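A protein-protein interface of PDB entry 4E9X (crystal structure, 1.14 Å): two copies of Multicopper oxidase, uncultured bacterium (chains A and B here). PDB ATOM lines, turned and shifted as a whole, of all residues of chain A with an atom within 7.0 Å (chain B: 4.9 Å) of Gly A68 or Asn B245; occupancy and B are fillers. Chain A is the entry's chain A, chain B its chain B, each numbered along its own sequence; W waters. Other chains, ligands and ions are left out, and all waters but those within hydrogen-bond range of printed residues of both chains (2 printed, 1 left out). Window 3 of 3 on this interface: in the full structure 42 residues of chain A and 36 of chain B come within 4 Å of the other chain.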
ATOM      1  N   VAL A  64       0.507  -7.572   7.918  1.00  0.00           N
ATOM      2  CA  VAL A  64       0.545  -8.765   7.066  1.00  0.00           C
ATOM      3  C   VAL A  64       1.975  -9.120   6.810  1.00  0.00           C
ATOM      4  O   VAL A  64       2.791  -8.284   6.380  1.00  0.00           O
ATOM      5  CB  VAL A  64      -0.185  -8.457   5.722  1.00  0.00           C
ATOM      6  CG1 VAL A  64      -0.022  -9.570   4.704  1.00  0.00           C
ATOM      7  CG2 VAL A  64      -1.680  -8.212   6.015  1.00  0.00           C
ATOM      8  N   HIS A  65       2.385 -10.354   7.113  1.00  0.00           N
ATOM      9  CA  HIS A  65       3.815 -10.622   6.972  1.00  0.00           C
ATOM     10  C   HIS A  65       4.306 -10.654   5.543  1.00  0.00           C
ATOM     11  O   HIS A  65       5.509 -10.468   5.322  1.00  0.00           O
ATOM     12  CB  HIS A  65       4.070 -12.031   7.559  1.00  0.00           C
ATOM     13  CG  HIS A  65       3.937 -12.104   9.041  1.00  0.00           C
ATOM     14  ND1 HIS A  65       3.858 -13.314   9.739  1.00  0.00           N
ATOM     15  CD2 HIS A  65       3.946 -11.112   9.947  1.00  0.00           C
ATOM     16  CE1 HIS A  65       3.796 -13.045  11.015  1.00  0.00           C
ATOM     17  NE2 HIS A  65       3.844 -11.728  11.187  1.00  0.00           N
ATOM     18  N   GLN A  66       3.411 -10.945   4.597  1.00  0.00           N
ATOM     19  CA  GLN A  66       3.802 -11.132   3.197  1.00  0.00           C
ATOM     20  C   GLN A  66       4.826 -12.253   3.072  1.00  0.00           C
ATOM     21  O   GLN A  66       5.852 -12.102   2.458  1.00  0.00           O
ATOM     22  CB  GLN A  66       4.376  -9.841   2.572  1.00  0.00           C
ATOM     23  CG  GLN A  66       3.381  -8.684   2.680  1.00  0.00           C
ATOM     24  CD  GLN A  66       2.196  -8.793   1.710  1.00  0.00           C
ATOM     25  OE1 GLN A  66       2.097  -9.689   0.884  1.00  0.00           O
ATOM     26  NE2 GLN A  66       1.279  -7.842   1.881  1.00  0.00           N
ATOM     27  N   LYS A  67       4.508 -13.388   3.675  1.00  0.00           N
ATOM     28  CA  LYS A  67       5.363 -14.561   3.690  1.00  0.00           C
ATOM     29  C   LYS A  67       5.500 -15.081   2.262  1.00  0.00           C
ATOM     30  O   LYS A  67       4.541 -15.649   1.712  1.00  0.00           O
ATOM     31  CB  LYS A  67       4.788 -15.630   4.621  1.00  0.00           C
ATOM     32  CG  LYS A  67       5.614 -16.838   4.939  1.00  0.00           C
ATOM     33  CD  LYS A  67       7.045 -16.527   5.366  1.00  0.00           C
ATOM     34  CE  LYS A  67       7.522 -17.319   6.571  1.00  0.00           C
ATOM     35  NZ  LYS A  67       7.049 -16.681   7.852  1.00  0.00           N
ATOM     36  N   GLY A  68       6.666 -14.867   1.673  1.00  0.00           N
ATOM     37  CA  GLY A  68       6.983 -15.272   0.321  1.00  0.00           C
ATOM     38  C   GLY A  68       6.273 -14.390  -0.697  1.00  0.00           C
ATOM     39  O   GLY A  68       6.222 -14.727  -1.878  1.00  0.00           O
ATOM     40  N   THR A  69       5.700 -13.297  -0.246  1.00  0.00           N
ATOM     41  CA  THR A  69       4.951 -12.401  -1.143  1.00  0.00           C
ATOM     42  C   THR A  69       5.396 -10.947  -0.940  1.00  0.00           C
ATOM     43  O   THR A  69       4.555 -10.031  -1.090  1.00  0.00           O
ATOM     44  CB  THR A  69       3.421 -12.489  -1.015  1.00  0.00           C
ATOM     45  OG1 THR A  69       3.008 -12.160   0.305  1.00  0.00           O
ATOM     46  CG2 THR A  69       3.001 -13.936  -1.228  1.00  0.00           C
ATOM     47  N   TRP A  70       6.695 -10.759  -0.650  1.00  0.00           N
ATOM     48  CA  TRP A  70       7.124  -9.396  -0.322  1.00  0.00           C
ATOM     49  C   TRP A  70       6.833  -8.361  -1.396  1.00  0.00           C
ATOM     50  O   TRP A  70       6.733  -7.155  -1.113  1.00  0.00           O
ATOM     51  CB  TRP A  70       8.639  -9.383   0.016  1.00  0.00           C
ATOM     52  CG  TRP A  70       9.563  -9.725  -1.144  1.00  0.00           C
ATOM     53  CD1 TRP A  70       9.924 -10.967  -1.528  1.00  0.00           C
ATOM     54  CD2 TRP A  70      10.214  -8.818  -2.014  1.00  0.00           C
ATOM     55  NE1 TRP A  70      10.776 -10.911  -2.621  1.00  0.00           N
ATOM     56  CE2 TRP A  70      10.967  -9.586  -2.932  1.00  0.00           C
ATOM     57  CE3 TRP A  70      10.244  -7.406  -2.134  1.00  0.00           C
ATOM     58  CZ2 TRP A  70      11.738  -8.997  -3.937  1.00  0.00           C
ATOM     59  CZ3 TRP A  70      11.015  -6.829  -3.138  1.00  0.00           C
ATOM     60  CH2 TRP A  70      11.760  -7.646  -4.038  1.00  0.00           C
ATOM     61  N   ARG A  71       6.709  -8.754  -2.671  1.00  0.00           N
ATOM     62  CA  ARG A  71       6.422  -7.815  -3.758  1.00  0.00           C
ATOM     63  C   ARG A  71       5.010  -7.253  -3.676  1.00  0.00           C
ATOM     64  O   ARG A  71       4.695  -6.318  -4.465  1.00  0.00           O
ATOM     65  CB  ARG A  71       6.735  -8.416  -5.140  1.00  0.00           C
ATOM     66  CG  ARG A  71       8.242  -8.762  -5.282  1.00  0.00           C
ATOM     67  CD  ARG A  71       8.504  -9.451  -6.647  1.00  0.00           C
ATOM     68  NE  ARG A  71       8.648  -8.474  -7.674  1.00  0.00           N
ATOM     69  CZ  ARG A  71       9.711  -7.701  -7.926  1.00  0.00           C
ATOM     70  NH1 ARG A  71      10.796  -7.833  -7.189  1.00  0.00           N
ATOM     71  NH2 ARG A  71       9.706  -6.817  -8.918  1.00  0.00           N
ATOM     72  N   GLY B 207       7.037  -7.019   7.367  1.00  0.00           N
ATOM     73  CA  GLY B 207       7.353  -8.378   7.028  1.00  0.00           C
ATOM     74  C   GLY B 207       7.550  -9.301   8.214  1.00  0.00           C
ATOM     75  O   GLY B 207       7.829 -10.510   8.019  1.00  0.00           O
ATOM     76  N   HIS B 208       7.543  -8.758   9.447  1.00  0.00           N
ATOM     77  CA  HIS B 208       7.972  -9.474  10.614  1.00  0.00           C
ATOM     78  C   HIS B 208       7.274  -8.920  11.858  1.00  0.00           C
ATOM     79  O   HIS B 208       7.111  -7.734  11.947  1.00  0.00           O
ATOM     80  CB  HIS B 208       9.475  -9.306  10.917  1.00  0.00           C
ATOM     81  CG  HIS B 208      10.399  -9.692   9.741  1.00  0.00           C
ATOM     82  ND1 HIS B 208      10.530  -8.817   8.659  1.00  0.00           N
ATOM     83  CD2 HIS B 208      11.149 -10.783   9.464  1.00  0.00           C
ATOM     84  CE1 HIS B 208      11.373  -9.418   7.794  1.00  0.00           C
ATOM     85  NE2 HIS B 208      11.743 -10.589   8.243  1.00  0.00           N
ATOM     86  N   ALA B 243      14.554 -13.921  11.264  1.00  0.00           N
ATOM     87  CA  ALA B 243      14.653 -13.564   9.851  1.00  0.00           C
ATOM     88  C   ALA B 243      14.282 -14.735   8.956  1.00  0.00           C
ATOM     89  O   ALA B 243      15.130 -15.410   8.341  1.00  0.00           O
ATOM     90  CB  ALA B 243      16.066 -13.044   9.544  1.00  0.00           C
ATOM     91  N   ASP B 244      12.998 -15.021   8.904  1.00  0.00           N
ATOM     92  CA  ASP B 244      12.548 -16.238   8.203  1.00  0.00           C
ATOM     93  C   ASP B 244      11.632 -15.890   7.018  1.00  0.00           C
ATOM     94  O   ASP B 244      10.889 -16.744   6.524  1.00  0.00           O
ATOM     95  CB  ASP B 244      11.825 -17.170   9.154  1.00  0.00           C
ATOM     96  CG  ASP B 244      10.618 -16.515   9.786  1.00  0.00           C
ATOM     97  OD1 ASP B 244      10.179 -15.398   9.451  1.00  0.00           O
ATOM     98  OD2 ASP B 244      10.061 -17.175  10.682  1.00  0.00           O
ATOM     99  N   ASN B 245      11.754 -14.635   6.531  1.00  0.00           N
ATOM    100  CA  ASN B 245      10.832 -14.207   5.454  1.00  0.00           C
ATOM    101  C   ASN B 245      11.578 -13.396   4.429  1.00  0.00           C
ATOM    102  O   ASN B 245      11.538 -12.142   4.457  1.00  0.00           O
ATOM    103  CB  ASN B 245       9.674 -13.408   6.107  1.00  0.00           C
ATOM    104  CG  ASN B 245       8.650 -12.998   5.076  1.00  0.00           C
ATOM    105  OD1 ASN B 245       8.611 -13.537   3.982  1.00  0.00           O
ATOM    106  ND2 ASN B 245       7.809 -12.012   5.414  1.00  0.00           N
ATOM    107  N   PRO B 246      12.335 -14.016   3.518  1.00  0.00           N
ATOM    108  CA  PRO B 246      13.195 -13.215   2.630  1.00  0.00           C
ATOM    109  C   PRO B 246      12.413 -12.239   1.754  1.00  0.00           C
ATOM    110  O   PRO B 246      11.384 -12.572   1.140  1.00  0.00           O
ATOM    111  CB  PRO B 246      13.870 -14.277   1.760  1.00  0.00           C
ATOM    112  CG  PRO B 246      13.818 -15.554   2.562  1.00  0.00           C
ATOM    113  CD  PRO B 246      12.531 -15.464   3.393  1.00  0.00           C
ATOM    114  N   GLY B 247      12.948 -11.028   1.681  1.00  0.00           N
ATOM    115  CA  GLY B 247      12.437  -9.971   0.860  1.00  0.00           C
ATOM    116  C   GLY B 247      13.207  -8.700   1.139  1.00  0.00           C
ATOM    117  O   GLY B 247      14.251  -8.771   1.757  1.00  0.00           O
ATOM    118  N   PHE B 249      12.258  -5.450   3.270  1.00  0.00           N
ATOM    119  CA  PHE B 249      11.184  -5.041   4.168  1.00  0.00           C
ATOM    120  C   PHE B 249      11.607  -3.791   4.909  1.00  0.00           C
ATOM    121  O   PHE B 249      12.517  -3.809   5.771  1.00  0.00           O
ATOM    122  CB  PHE B 249      10.850  -6.141   5.162  1.00  0.00           C
ATOM    123  CG  PHE B 249      10.012  -7.260   4.514  1.00  0.00           C
ATOM    124  CD1 PHE B 249       8.700  -6.957   4.119  1.00  0.00           C
ATOM    125  CD2 PHE B 249      10.510  -8.546   4.313  1.00  0.00           C
ATOM    126  CE1 PHE B 249       7.896  -7.929   3.551  1.00  0.00           C
ATOM    127  CE2 PHE B 249       9.687  -9.523   3.752  1.00  0.00           C
ATOM    128  CZ  PHE B 249       8.358  -9.212   3.404  1.00  0.00           C
ATOM    129  N   TYR B 275      17.324  -9.026   2.717  1.00  0.00           N
ATOM    130  CA  TYR B 275      17.852 -10.398   2.832  1.00  0.00           C
ATOM    131  C   TYR B 275      18.815 -10.700   1.705  1.00  0.00           C
ATOM    132  O   TYR B 275      18.574 -10.357   0.530  1.00  0.00           O
ATOM    133  CB  TYR B 275      16.719 -11.396   2.737  1.00  0.00           C
ATOM    134  CG  TYR B 275      15.847 -11.596   3.967  1.00  0.00           C
ATOM    135  CD1 TYR B 275      15.003 -10.615   4.454  1.00  0.00           C
ATOM    136  CD2 TYR B 275      15.869 -12.809   4.646  1.00  0.00           C
ATOM    137  CE1 TYR B 275      14.212 -10.825   5.598  1.00  0.00           C
ATOM    138  CE2 TYR B 275      15.091 -13.077   5.764  1.00  0.00           C
ATOM    139  CZ  TYR B 275      14.253 -12.032   6.228  1.00  0.00           C
ATOM    140  OH  TYR B 275      13.488 -12.361   7.295  1.00  0.00           O
HETATM  141  O   HOH W   1       4.661  -6.286   6.028  1.00  0.00           O
HETATM  142  O   HOH W   2       9.215 -15.890   2.596  1.00  0.00           O
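The side-chain hydroxyl (OG1) of Thr A69 is in hydrogen-bond range of the side-chain amide oxygen (OE1) of Gln A66 (2.7 Å).
ND2 of Asn B245 sits at hydrogen-bond distance from O of Gly B207.
The backbone NH (N) of Asp B244 lies within hydrogen-bond range of the side-chain hydroxyl (OH) of Tyr B275 (3.1 Å).
The backbone NH (N) of Asn B245 is in hydrogen-bond range of the side-chain hydroxyl (OH) of Tyr B275.
The backbone carbonyl oxygen (O) of Gly B247 sits at hydrogen-bond distance from the backbone NH (N) of Tyr B275, at 3.2 Å.
No position is printed for both chains.
Of the 11 pairs that touch across the chains among the printed residues, none has its exchanged pair printed and touching as well.
Hydrophobic or aromatic side chains of chain A that line the printed part of chain B: Trp A70.
Printed residues of chain B that touch a printed residue of chain A: Gly B207, Asp B244, Asn B245, Pro B246, Gly B247 and Phe B249.
Hydrophobic or aromatic side chains of chain B that line the printed part of chain A: Phe B249.
Among the printed residues, 11 pairs touch across the chains.
Water W1 bridges O of Val A64 (2.8 Å) and N of Gly B207 (2.8 Å).
Water W2 lies within hydrogen-bond range of OD1 of Asn B245 (2.8 Å) and N of Gly A68 (2.9 Å).
O of His A65 sits at hydrogen-bond distance from ND2 of Asn B245, 2.8 Å away.
The side-chain amide oxygen of Asn B245 lies close to the backbone carbonyl oxygen of Gln A66.
The side-chain amino group (NZ) of Lys A67 is in salt-bridge range of the side-chain carboxylate (OD1) of Asp B244 (3.7 Å).
The side-chain amide oxygen (OD1) of Asn B245 sits at hydrogen-bond distance from the backbone NH (N) of Gly A68 (3.3 Å).
Printed residues of chain B within 4 Å of His A65: Gly B207 (3.3 Å), Asn B245 (2.8 Å) and Phe B249 (3.7 Å).
Of the printed residues of chain B, Gln A66 touches Asn B245 and Phe B249.
Gly A68 touches just one residue of chain B: Asn B245.
Ala B243 touches none of the printed residues of chain A.
Of the printed residues of chain A, Pro B246 touches Trp A70 (3.4 Å).
Printed residues of chain A within 4 Å of Gly B247: Trp A70.
Of the printed residues of chain A, Phe B249 touches His A65, Gln A66 and Trp A70.
Tyr B275 touches none of the printed residues of chain A.
The nearest printed residue of chain B that does not touch Gln A66 is Gly B207 (5.3 Å).
Gly B207 touches His A65.
O of His A65 touches CZ of Phe B249, 3.7 Å away.
Gln A66 touches Phe B249 (O to CZ, 3.9 Å).
Lys A67 touches Asn B245.
CD1 of Trp A70 touches O of Pro B246 (3.4 Å).
Gly B247 touches Trp A70.
Trp A70 touches Phe B249.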
